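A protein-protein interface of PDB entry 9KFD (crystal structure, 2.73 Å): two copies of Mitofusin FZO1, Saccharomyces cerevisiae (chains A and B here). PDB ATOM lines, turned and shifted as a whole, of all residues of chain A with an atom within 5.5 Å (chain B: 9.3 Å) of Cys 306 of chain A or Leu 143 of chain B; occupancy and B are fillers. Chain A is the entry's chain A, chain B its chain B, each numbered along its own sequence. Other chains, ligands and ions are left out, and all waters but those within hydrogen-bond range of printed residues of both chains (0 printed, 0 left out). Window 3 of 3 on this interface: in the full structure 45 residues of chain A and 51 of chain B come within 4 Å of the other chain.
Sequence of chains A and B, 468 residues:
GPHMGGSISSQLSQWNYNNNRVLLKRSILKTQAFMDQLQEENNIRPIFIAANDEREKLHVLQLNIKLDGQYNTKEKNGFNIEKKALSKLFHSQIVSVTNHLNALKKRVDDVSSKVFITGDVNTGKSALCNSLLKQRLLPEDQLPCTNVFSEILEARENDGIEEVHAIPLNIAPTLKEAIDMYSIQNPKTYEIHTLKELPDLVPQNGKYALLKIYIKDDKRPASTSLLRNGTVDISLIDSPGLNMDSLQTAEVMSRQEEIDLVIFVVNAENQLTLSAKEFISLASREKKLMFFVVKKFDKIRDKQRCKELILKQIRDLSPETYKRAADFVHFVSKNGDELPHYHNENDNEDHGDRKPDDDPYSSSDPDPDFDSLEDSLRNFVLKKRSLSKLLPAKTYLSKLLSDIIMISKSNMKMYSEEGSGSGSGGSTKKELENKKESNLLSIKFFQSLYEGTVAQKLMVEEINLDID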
ATOM      1  N   ALA A 268     -11.022 -27.697  -4.007  1.00  0.00           N
ATOM      2  CA  ALA A 268     -11.642 -27.057  -2.850  1.00  0.00           C
ATOM      3  C   ALA A 268     -11.673 -27.969  -1.628  1.00  0.00           C
ATOM      4  O   ALA A 268     -11.549 -27.487  -0.497  1.00  0.00           O
ATOM      5  CB  ALA A 268     -13.058 -26.599  -3.204  1.00  0.00           C
ATOM      6  N   GLU A 269     -11.839 -29.280  -1.827  1.00  0.00           N
ATOM      7  CA  GLU A 269     -11.891 -30.193  -0.690  1.00  0.00           C
ATOM      8  C   GLU A 269     -10.527 -30.317  -0.021  1.00  0.00           C
ATOM      9  O   GLU A 269     -10.414 -30.217   1.207  1.00  0.00           O
ATOM     10  CB  GLU A 269     -12.385 -31.572  -1.127  1.00  0.00           C
ATOM     11  CG  GLU A 269     -13.523 -31.568  -2.126  1.00  0.00           C
ATOM     12  CD  GLU A 269     -13.954 -32.976  -2.495  1.00  0.00           C
ATOM     13  OE1 GLU A 269     -13.081 -33.869  -2.546  1.00  0.00           O
ATOM     14  OE2 GLU A 269     -15.163 -33.191  -2.726  1.00  0.00           O
ATOM     15  N   GLN A 271      -7.873 -28.370  -0.321  1.00  0.00           N
ATOM     16  CA  GLN A 271      -7.186 -27.091  -0.094  1.00  0.00           C
ATOM     17  C   GLN A 271      -5.785 -27.200  -0.705  1.00  0.00           C
ATOM     18  O   GLN A 271      -5.571 -27.964  -1.655  1.00  0.00           O
ATOM     19  CB  GLN A 271      -7.221 -26.735   1.383  1.00  0.00           C
ATOM     20  CG  GLN A 271      -8.540 -27.088   2.052  1.00  0.00           C
ATOM     21  CD  GLN A 271      -8.472 -27.033   3.562  1.00  0.00           C
ATOM     22  OE1 GLN A 271      -9.495 -27.127   4.239  1.00  0.00           O
ATOM     23  NE2 GLN A 271      -7.267 -26.878   4.099  1.00  0.00           N
ATOM     24  N   PHE A 297     -15.628 -25.967  -6.120  1.00  0.00           N
ATOM     25  CA  PHE A 297     -16.154 -25.310  -4.933  1.00  0.00           C
ATOM     26  C   PHE A 297     -17.649 -25.535  -4.768  1.00  0.00           C
ATOM     27  O   PHE A 297     -18.168 -25.374  -3.657  1.00  0.00           O
ATOM     28  CB  PHE A 297     -15.860 -23.808  -4.989  1.00  0.00           C
ATOM     29  CG  PHE A 297     -16.127 -23.087  -3.698  1.00  0.00           C
ATOM     30  CD1 PHE A 297     -15.419 -23.407  -2.550  1.00  0.00           C
ATOM     31  CD2 PHE A 297     -17.081 -22.084  -3.634  1.00  0.00           C
ATOM     32  CE1 PHE A 297     -15.660 -22.742  -1.361  1.00  0.00           C
ATOM     33  CE2 PHE A 297     -17.327 -21.418  -2.447  1.00  0.00           C
ATOM     34  CZ  PHE A 297     -16.615 -21.746  -1.311  1.00  0.00           C
ATOM     35  N   ILE A 300     -18.548 -28.089  -2.020  1.00  0.00           N
ATOM     36  CA  ILE A 300     -18.309 -27.794  -0.612  1.00  0.00           C
ATOM     37  C   ILE A 300     -19.592 -27.288   0.034  1.00  0.00           C
ATOM     38  O   ILE A 300     -20.280 -26.417  -0.512  1.00  0.00           O
ATOM     39  CB  ILE A 300     -17.171 -26.773  -0.462  1.00  0.00           C
ATOM     40  CG1 ILE A 300     -15.868 -27.315  -1.060  1.00  0.00           C
ATOM     41  CG2 ILE A 300     -16.965 -26.408   1.000  1.00  0.00           C
ATOM     42  CD1 ILE A 300     -15.614 -28.785  -0.790  1.00  0.00           C
ATOM     43  N   ASP A 302     -19.417 -26.510   3.549  1.00  0.00           N
ATOM     44  CA  ASP A 302     -18.960 -25.642   4.627  1.00  0.00           C
ATOM     45  C   ASP A 302     -18.125 -24.520   4.024  1.00  0.00           C
ATOM     46  O   ASP A 302     -16.961 -24.331   4.392  1.00  0.00           O
ATOM     47  CB  ASP A 302     -18.163 -26.442   5.660  1.00  0.00           C
ATOM     48  CG  ASP A 302     -18.326 -25.901   7.069  1.00  0.00           C
ATOM     49  OD1 ASP A 302     -18.408 -24.665   7.230  1.00  0.00           O
ATOM     50  OD2 ASP A 302     -18.382 -26.718   8.014  1.00  0.00           O
ATOM     51  N   LYS A 303     -18.731 -23.771   3.096  1.00  0.00           N
ATOM     52  CA  LYS A 303     -17.977 -22.871   2.228  1.00  0.00           C
ATOM     53  C   LYS A 303     -17.205 -21.822   3.020  1.00  0.00           C
ATOM     54  O   LYS A 303     -16.052 -21.516   2.691  1.00  0.00           O
ATOM     55  CB  LYS A 303     -18.922 -22.194   1.234  1.00  0.00           C
ATOM     56  CG  LYS A 303     -19.496 -23.123   0.176  1.00  0.00           C
ATOM     57  CD  LYS A 303     -20.493 -22.388  -0.706  1.00  0.00           C
ATOM     58  CE  LYS A 303     -21.373 -23.352  -1.489  1.00  0.00           C
ATOM     59  NZ  LYS A 303     -20.578 -24.426  -2.146  1.00  0.00           N
ATOM     60  N   GLN A 304     -17.821 -21.259   4.061  1.00  0.00           N
ATOM     61  CA  GLN A 304     -17.176 -20.184   4.810  1.00  0.00           C
ATOM     62  C   GLN A 304     -15.891 -20.665   5.478  1.00  0.00           C
ATOM     63  O   GLN A 304     -14.853 -19.997   5.404  1.00  0.00           O
ATOM     64  CB  GLN A 304     -18.145 -19.615   5.848  1.00  0.00           C
ATOM     65  CG  GLN A 304     -17.583 -18.452   6.647  1.00  0.00           C
ATOM     66  CD  GLN A 304     -18.166 -18.370   8.043  1.00  0.00           C
ATOM     67  OE1 GLN A 304     -17.462 -18.563   9.036  1.00  0.00           O
ATOM     68  NE2 GLN A 304     -19.461 -18.083   8.128  1.00  0.00           N
ATOM     69  N   ARG A 305     -15.940 -21.822   6.139  1.00  0.00           N
ATOM     70  CA  ARG A 305     -14.729 -22.363   6.751  1.00  0.00           C
ATOM     71  C   ARG A 305     -13.706 -22.760   5.693  1.00  0.00           C
ATOM     72  O   ARG A 305     -12.505 -22.509   5.855  1.00  0.00           O
ATOM     73  CB  ARG A 305     -15.078 -23.558   7.638  1.00  0.00           C
ATOM     74  CG  ARG A 305     -13.913 -24.503   7.880  1.00  0.00           C
ATOM     75  CD  ARG A 305     -14.156 -25.425   9.063  1.00  0.00           C
ATOM     76  NE  ARG A 305     -15.242 -26.368   8.823  1.00  0.00           N
ATOM     77  CZ  ARG A 305     -15.071 -27.662   8.591  1.00  0.00           C
ATOM     78  NH1 ARG A 305     -13.862 -28.198   8.529  1.00  0.00           N
ATOM     79  NH2 ARG A 305     -16.137 -28.437   8.414  1.00  0.00           N
ATOM     80  N   CYS A 306     -14.165 -23.391   4.608  1.00  0.00           N
ATOM     81  CA  CYS A 306     -13.268 -23.720   3.504  1.00  0.00           C
ATOM     82  C   CYS A 306     -12.670 -22.457   2.892  1.00  0.00           C
ATOM     83  O   CYS A 306     -11.472 -22.421   2.591  1.00  0.00           O
ATOM     84  CB  CYS A 306     -14.017 -24.536   2.449  1.00  0.00           C
ATOM     85  SG  CYS A 306     -13.100 -24.847   0.925  1.00  0.00           S
ATOM     86  N   LYS A 307     -13.508 -21.424   2.686  1.00  0.00           N
ATOM     87  CA  LYS A 307     -13.054 -20.081   2.305  1.00  0.00           C
ATOM     88  C   LYS A 307     -11.815 -19.673   3.074  1.00  0.00           C
ATOM     89  O   LYS A 307     -10.753 -19.436   2.492  1.00  0.00           O
ATOM     90  CB  LYS A 307     -14.128 -19.042   2.620  1.00  0.00           C
ATOM     91  CG  LYS A 307     -14.227 -17.916   1.673  1.00  0.00           C
ATOM     92  CD  LYS A 307     -14.754 -18.503   0.377  1.00  0.00           C
ATOM     93  CE  LYS A 307     -13.970 -18.051  -0.827  1.00  0.00           C
ATOM     94  NZ  LYS A 307     -14.513 -18.840  -1.943  1.00  0.00           N
ATOM     95  N   GLU A 308     -11.956 -19.544   4.397  1.00  0.00           N
ATOM     96  CA  GLU A 308     -10.899 -18.987   5.232  1.00  0.00           C
ATOM     97  C   GLU A 308      -9.653 -19.860   5.227  1.00  0.00           C
ATOM     98  O   GLU A 308      -8.534 -19.353   5.370  1.00  0.00           O
ATOM     99  CB  GLU A 308     -11.429 -18.809   6.655  1.00  0.00           C
ATOM    100  CG  GLU A 308     -10.502 -18.091   7.597  1.00  0.00           C
ATOM    101  CD  GLU A 308     -11.162 -17.781   8.924  1.00  0.00           C
ATOM    102  OE1 GLU A 308     -10.642 -16.902   9.638  1.00  0.00           O
ATOM    103  OE2 GLU A 308     -12.197 -18.409   9.253  1.00  0.00           O
ATOM    104  N   LEU A 309      -9.826 -21.170   5.056  1.00  0.00           N
ATOM    105  CA  LEU A 309      -8.684 -22.071   5.111  1.00  0.00           C
ATOM    106  C   LEU A 309      -7.770 -21.889   3.905  1.00  0.00           C
ATOM    107  O   LEU A 309      -6.542 -21.935   4.044  1.00  0.00           O
ATOM    108  CB  LEU A 309      -9.169 -23.517   5.228  1.00  0.00           C
ATOM    109  CG  LEU A 309      -9.526 -23.944   6.658  1.00  0.00           C
ATOM    110  CD1 LEU A 309     -10.145 -25.331   6.692  1.00  0.00           C
ATOM    111  CD2 LEU A 309      -8.301 -23.885   7.561  1.00  0.00           C
ATOM    112  N   ILE A 310      -8.338 -21.667   2.716  1.00  0.00           N
ATOM    113  CA  ILE A 310      -7.503 -21.445   1.536  1.00  0.00           C
ATOM    114  C   ILE A 310      -6.758 -20.120   1.653  1.00  0.00           C
ATOM    115  O   ILE A 310      -5.549 -20.045   1.405  1.00  0.00           O
ATOM    116  CB  ILE A 310      -8.340 -21.492   0.244  1.00  0.00           C
ATOM    117  CG1 ILE A 310      -9.442 -22.545   0.326  1.00  0.00           C
ATOM    118  CG2 ILE A 310      -7.440 -21.759  -0.956  1.00  0.00           C
ATOM    119  CD1 ILE A 310      -8.959 -23.950   0.148  1.00  0.00           C
ATOM    120  N   LEU A 311      -7.475 -19.054   2.021  1.00  0.00           N
ATOM    121  CA  LEU A 311      -6.854 -17.735   2.104  1.00  0.00           C
ATOM    122  C   LEU A 311      -5.741 -17.712   3.143  1.00  0.00           C
ATOM    123  O   LEU A 311      -4.667 -17.149   2.900  1.00  0.00           O
ATOM    124  CB  LEU A 311      -7.913 -16.680   2.427  1.00  0.00           C
ATOM    125  CG  LEU A 311      -8.908 -16.358   1.310  1.00  0.00           C
ATOM    126  CD1 LEU A 311      -9.824 -15.217   1.718  1.00  0.00           C
ATOM    127  CD2 LEU A 311      -8.171 -16.018   0.023  1.00  0.00           C
ATOM    128  N   VAL B 121      -5.160 -37.560   2.179  1.00  0.00           N
ATOM    129  CA  VAL B 121      -6.189 -36.756   2.820  1.00  0.00           C
ATOM    130  C   VAL B 121      -7.520 -36.963   2.109  1.00  0.00           C
ATOM    131  O   VAL B 121      -7.581 -37.083   0.877  1.00  0.00           O
ATOM    132  CB  VAL B 121      -5.775 -35.274   2.832  1.00  0.00           C
ATOM    133  CG1 VAL B 121      -5.586 -34.753   1.412  1.00  0.00           C
ATOM    134  CG2 VAL B 121      -6.798 -34.431   3.584  1.00  0.00           C
ATOM    135  N   ASN B 122      -8.593 -37.045   2.898  1.00  0.00           N
ATOM    136  CA  ASN B 122      -9.962 -37.104   2.378  1.00  0.00           C
ATOM    137  C   ASN B 122     -10.191 -38.344   1.515  1.00  0.00           C
ATOM    138  O   ASN B 122     -10.905 -38.298   0.512  1.00  0.00           O
ATOM    139  CB  ASN B 122     -10.306 -35.832   1.599  1.00  0.00           C
ATOM    140  CG  ASN B 122     -10.457 -34.623   2.497  1.00  0.00           C
ATOM    141  OD1 ASN B 122     -10.855 -34.745   3.656  1.00  0.00           O
ATOM    142  ND2 ASN B 122     -10.138 -33.445   1.969  1.00  0.00           N
ATOM    143  N   THR B 123      -9.580 -39.463   1.902  1.00  0.00           N
ATOM    144  CA  THR B 123      -9.822 -40.725   1.212  1.00  0.00           C
ATOM    145  C   THR B 123     -10.917 -41.556   1.864  1.00  0.00           C
ATOM    146  O   THR B 123     -11.514 -42.403   1.192  1.00  0.00           O
ATOM    147  CB  THR B 123      -8.541 -41.562   1.143  1.00  0.00           C
ATOM    148  OG1 THR B 123      -7.876 -41.528   2.411  1.00  0.00           O
ATOM    149  CG2 THR B 123      -7.611 -41.029   0.065  1.00  0.00           C
ATOM    150  N   LYS B 125     -10.457 -42.501   5.512  1.00  0.00           N
ATOM    151  CA  LYS B 125      -9.788 -43.260   6.565  1.00  0.00           C
ATOM    152  C   LYS B 125     -10.656 -43.355   7.814  1.00  0.00           C
ATOM    153  O   LYS B 125     -10.843 -44.441   8.374  1.00  0.00           O
ATOM    154  CB  LYS B 125      -8.436 -42.625   6.897  1.00  0.00           C
ATOM    155  CG  LYS B 125      -7.471 -42.560   5.727  1.00  0.00           C
ATOM    156  CD  LYS B 125      -6.266 -41.688   6.053  1.00  0.00           C
ATOM    157  CE  LYS B 125      -6.684 -40.295   6.502  1.00  0.00           C
ATOM    158  NZ  LYS B 125      -7.143 -39.452   5.369  1.00  0.00           N
ATOM    159  N   SER B 126     -11.194 -42.220   8.268  1.00  0.00           N
ATOM    160  CA  SER B 126     -12.042 -42.232   9.456  1.00  0.00           C
ATOM    161  C   SER B 126     -13.357 -42.952   9.190  1.00  0.00           C
ATOM    162  O   SER B 126     -13.853 -43.689  10.051  1.00  0.00           O
ATOM    163  CB  SER B 126     -12.301 -40.803   9.933  1.00  0.00           C
ATOM    164  OG  SER B 126     -11.103 -40.176  10.354  1.00  0.00           O
ATOM    165  N   PRO B 139     -14.570 -38.583  14.142  1.00  0.00           N
ATOM    166  CA  PRO B 139     -15.111 -37.463  13.363  1.00  0.00           C
ATOM    167  C   PRO B 139     -14.864 -37.649  11.874  1.00  0.00           C
ATOM    168  O   PRO B 139     -13.793 -38.089  11.450  1.00  0.00           O
ATOM    169  CB  PRO B 139     -14.351 -36.248  13.913  1.00  0.00           C
ATOM    170  CG  PRO B 139     -13.831 -36.688  15.247  1.00  0.00           C
ATOM    171  CD  PRO B 139     -13.540 -38.146  15.097  1.00  0.00           C
ATOM    172  N   GLU B 140     -15.878 -37.315  11.081  1.00  0.00           N
ATOM    173  CA  GLU B 140     -15.800 -37.339   9.629  1.00  0.00           C
ATOM    174  C   GLU B 140     -16.132 -35.955   9.095  1.00  0.00           C
ATOM    175  O   GLU B 140     -17.089 -35.320   9.552  1.00  0.00           O
ATOM    176  CB  GLU B 140     -16.763 -38.372   9.034  1.00  0.00           C
ATOM    177  CG  GLU B 140     -16.532 -39.796   9.506  1.00  0.00           C
ATOM    178  CD  GLU B 140     -17.556 -40.767   8.945  1.00  0.00           C
ATOM    179  OE1 GLU B 140     -18.279 -40.386   7.999  1.00  0.00           O
ATOM    180  OE2 GLU B 140     -17.638 -41.907   9.450  1.00  0.00           O
ATOM    181  N   ASP B 141     -15.342 -35.484   8.134  1.00  0.00           N
ATOM    182  CA  ASP B 141     -15.585 -34.173   7.553  1.00  0.00           C
ATOM    183  C   ASP B 141     -15.119 -34.157   6.106  1.00  0.00           C
ATOM    184  O   ASP B 141     -14.172 -34.854   5.730  1.00  0.00           O
ATOM    185  CB  ASP B 141     -14.886 -33.061   8.342  1.00  0.00           C
ATOM    186  CG  ASP B 141     -15.501 -31.698   8.088  1.00  0.00           C
ATOM    187  OD1 ASP B 141     -16.621 -31.450   8.582  1.00  0.00           O
ATOM    188  OD2 ASP B 141     -14.868 -30.878   7.389  1.00  0.00           O
ATOM    189  N   GLN B 142     -15.806 -33.346   5.297  1.00  0.00           N
ATOM    190  CA  GLN B 142     -15.428 -33.185   3.898  1.00  0.00           C
ATOM    191  C   GLN B 142     -14.041 -32.565   3.773  1.00  0.00           C
ATOM    192  O   GLN B 142     -13.219 -33.018   2.969  1.00  0.00           O
ATOM    193  CB  GLN B 142     -16.474 -32.331   3.181  1.00  0.00           C
ATOM    194  CG  GLN B 142     -16.259 -32.168   1.690  1.00  0.00           C
ATOM    195  CD  GLN B 142     -17.323 -31.293   1.052  1.00  0.00           C
ATOM    196  OE1 GLN B 142     -17.789 -30.323   1.653  1.00  0.00           O
ATOM    197  NE2 GLN B 142     -17.718 -31.637  -0.168  1.00  0.00           N
ATOM    198  N   LEU B 143     -13.768 -31.532   4.566  1.00  0.00           N
ATOM    199  CA  LEU B 143     -12.466 -30.891   4.607  1.00  0.00           C
ATOM    200  C   LEU B 143     -11.515 -31.694   5.494  1.00  0.00           C
ATOM    201  O   LEU B 143     -11.954 -32.555   6.260  1.00  0.00           O
ATOM    202  CB  LEU B 143     -12.614 -29.462   5.123  1.00  0.00           C
ATOM    203  CG  LEU B 143     -13.812 -28.676   4.583  1.00  0.00           C
ATOM    204  CD1 LEU B 143     -13.898 -27.309   5.243  1.00  0.00           C
ATOM    205  CD2 LEU B 143     -13.746 -28.540   3.068  1.00  0.00           C
ATOM    206  N   PRO B 144     -10.205 -31.447   5.392  1.00  0.00           N
ATOM    207  CA  PRO B 144      -9.244 -32.185   6.226  1.00  0.00           C
ATOM    208  C   PRO B 144      -9.617 -32.165   7.703  1.00  0.00           C
ATOM    209  O   PRO B 144      -9.840 -31.106   8.295  1.00  0.00           O
ATOM    210  CB  PRO B 144      -7.926 -31.452   5.967  1.00  0.00           C
ATOM    211  CG  PRO B 144      -8.063 -30.951   4.576  1.00  0.00           C
ATOM    212  CD  PRO B 144      -9.523 -30.630   4.371  1.00  0.00           C
ATOM    213  N   CYS B 145      -9.682 -33.359   8.295  1.00  0.00           N
ATOM    214  CA  CYS B 145     -10.142 -33.534   9.668  1.00  0.00           C
ATOM    215  C   CYS B 145      -9.051 -34.073  10.581  1.00  0.00           C
ATOM    216  O   CYS B 145      -8.454 -33.322  11.360  1.00  0.00           O
ATOM    217  CB  CYS B 145     -11.344 -34.479   9.708  1.00  0.00           C
ATOM    218  SG  CYS B 145     -12.469 -34.206  11.094  1.00  0.00           S
ATOM    219  N   THR B 146      -8.797 -35.377  10.495  1.00  0.00           N
ATOM    220  CA  THR B 146      -7.903 -36.043  11.434  1.00  0.00           C
ATOM    221  C   THR B 146      -6.480 -35.522  11.294  1.00  0.00           C
ATOM    222  O   THR B 146      -5.851 -35.673  10.242  1.00  0.00           O
ATOM    223  CB  THR B 146      -7.940 -37.553  11.209  1.00  0.00           C
ATOM    224  OG1 THR B 146      -9.275 -37.960  10.884  1.00  0.00           O
ATOM    225  CG2 THR B 146      -7.480 -38.287  12.460  1.00  0.00           C
ATOM    226  N   ASN B 147      -5.976 -34.906  12.364  1.00  0.00           N
ATOM    227  CA  ASN B 147      -4.587 -34.478  12.438  1.00  0.00           C
ATOM    228  C   ASN B 147      -3.794 -35.183  13.528  1.00  0.00           C
ATOM    229  O   ASN B 147      -2.559 -35.145  13.486  1.00  0.00           O
ATOM    230  CB  ASN B 147      -4.503 -32.961  12.664  1.00  0.00           C
ATOM    231  CG  ASN B 147      -4.943 -32.166  11.448  1.00  0.00           C
ATOM    232  OD1 ASN B 147      -4.922 -32.668  10.323  1.00  0.00           O
ATOM    233  ND2 ASN B 147      -5.350 -30.920  11.670  1.00  0.00           N
ATOM    234  N   PRO B 203      -8.176 -32.325  15.540  1.00  0.00           N
ATOM    235  CA  PRO B 203      -7.369 -31.420  14.711  1.00  0.00           C
ATOM    236  C   PRO B 203      -6.214 -30.736  15.430  1.00  0.00           C
ATOM    237  O   PRO B 203      -5.505 -29.948  14.793  1.00  0.00           O
ATOM    238  CB  PRO B 203      -8.404 -30.384  14.258  1.00  0.00           C
ATOM    239  CG  PRO B 203      -9.283 -30.251  15.418  1.00  0.00           C
ATOM    240  CD  PRO B 203      -9.398 -31.634  16.005  1.00  0.00           C
ATOM    241  N   MET B 244      -0.175 -33.502   3.211  1.00  0.00           N
ATOM    242  CA  MET B 244      -0.757 -32.335   3.864  1.00  0.00           C
ATOM    243  C   MET B 244       0.350 -31.455   4.427  1.00  0.00           C
ATOM    244  O   MET B 244       0.501 -30.296   4.042  1.00  0.00           O
ATOM    245  CB  MET B 244      -1.717 -32.756   4.980  1.00  0.00           C
ATOM    246  CG  MET B 244      -3.109 -33.149   4.505  1.00  0.00           C
ATOM    247  SD  MET B 244      -4.076 -31.687   3.643  1.00  0.00           S
ATOM    248  CE  MET B 244      -4.427 -30.589   5.218  1.00  0.00           C
ATOM    249  N   LYS B 296     -15.097 -44.109  -2.506  1.00  0.00           N
ATOM    250  CA  LYS B 296     -15.678 -43.178  -3.475  1.00  0.00           C
ATOM    251  C   LYS B 296     -15.755 -43.793  -4.870  1.00  0.00           C
ATOM    252  O   LYS B 296     -15.690 -43.083  -5.878  1.00  0.00           O
ATOM    253  CB  LYS B 296     -14.907 -41.855  -3.516  1.00  0.00           C
ATOM    254  CG  LYS B 296     -14.667 -41.232  -2.152  1.00  0.00           C
ATOM    255  CD  LYS B 296     -13.931 -39.909  -2.279  1.00  0.00           C
ATOM    256  CE  LYS B 296     -13.479 -39.399  -0.921  1.00  0.00           C
ATOM    257  NZ  LYS B 296     -14.623 -38.969  -0.072  1.00  0.00           N
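The side-chain sulfur (SG) of Cys 306 of chain A is in hydrogen-bond range of the backbone carbonyl oxygen (O) of Ala 268 of chain A (3.4 Å).
O of Ile 300 of chain A sits at hydrogen-bond distance from NZ of Lys 303 of chain A.
The guanidinium group (NH2) of Arg 305 of chain A is in salt-bridge range of the side-chain carboxylate (OD2) of Asp 302 of chain A (2.9 Å).
The side-chain amide oxygen of Asn 122 of chain B sits close to the backbone carbonyl oxygen of Gln 142 of chain B (3.0 Å).
The side-chain carboxylate (OD2) of Asp 141 of chain B is in hydrogen-bond range of the backbone NH (N) of Leu 143 of chain B (3.1 Å).
No position is printed for both chains.
Cys 306 of chain A touches one residue of chain B.
Printed residues of chain A within 4 Å of Leu 143 of chain B: Gln 271, Arg 305 and Cys 306.
Of the printed residues of chain B, Arg 305 of chain A touches Asp 141 and Leu 143.
Of the printed residues of chain A, Asp 141 of chain B touches Arg 305 (2.9 Å).
Of the printed residues of chain A, Asn 122 of chain B touches Glu 269 (3.3 Å).
Of the printed residues of chain B, Gln 271 of chain A touches Leu 143 (3.995 Å) and Pro 144 (3.5 Å).
Of the printed residues of chain B, Ile 300 of chain A touches Gln 142.
Of the printed residues of chain B, Glu 269 of chain A touches Asn 122 (3.3 Å), Gln 142 (3.9 Å) and Pro 144 (3.3 Å).
The nearest residue of chain B that does not touch Cys 306 of chain A is Gln 142 of chain B (7.0 Å).
The nearest printed residue of chain A that does not touch Gln 142 of chain B is Asp 302 of chain A (4.6 Å).
The backbone carbonyl oxygen of Glu 269 of chain A is in hydrogen-bond range of the side-chain amide nitrogen of Asn 122 of chain B.
The guanidinium group of Arg 305 of chain A lies within salt-bridge range of the side-chain carboxylate of Asp 141 of chain B (2.9 Å).
Printed residues of chain A that touch a printed residue of chain B: Glu 269, Gln 271, Ile 300, Arg 305 and Cys 306.
Hydrophobic or aromatic side chains of chain A that line the printed part of chain B: Ile 300.
Hydrophobic or aromatic side chains of chain B within 4 Å of the printed part of chain A: Leu 143 and Pro 144.
Among the printed residues, 9 pairs touch across the chains.
Among the printed residues, Asp or Glu carboxylates within 4 Å of a Lys or Arg side-chain nitrogen of the other chain: Arg 305 of chain A with Asp 141 of chain B.
Among the printed residues, pairs that only touch across the chains: Glu 269 of chain A with Gln 142 of chain B (3.9 Å), Glu 269 of chain A with Pro 144 of chain B (3.3 Å), Gln 271 of chain A with Leu 143 of chain B (3.995 Å), Gln 271 of chain A with Pro 144 of chain B (3.5 Å), Ile 300 of chain A with Gln 142 of chain B (3.4 Å), Arg 305 of chain A with Leu 143 of chain B (3.4 Å) and Cys 306 of chain A with Leu 143 of chain B (3.9 Å).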
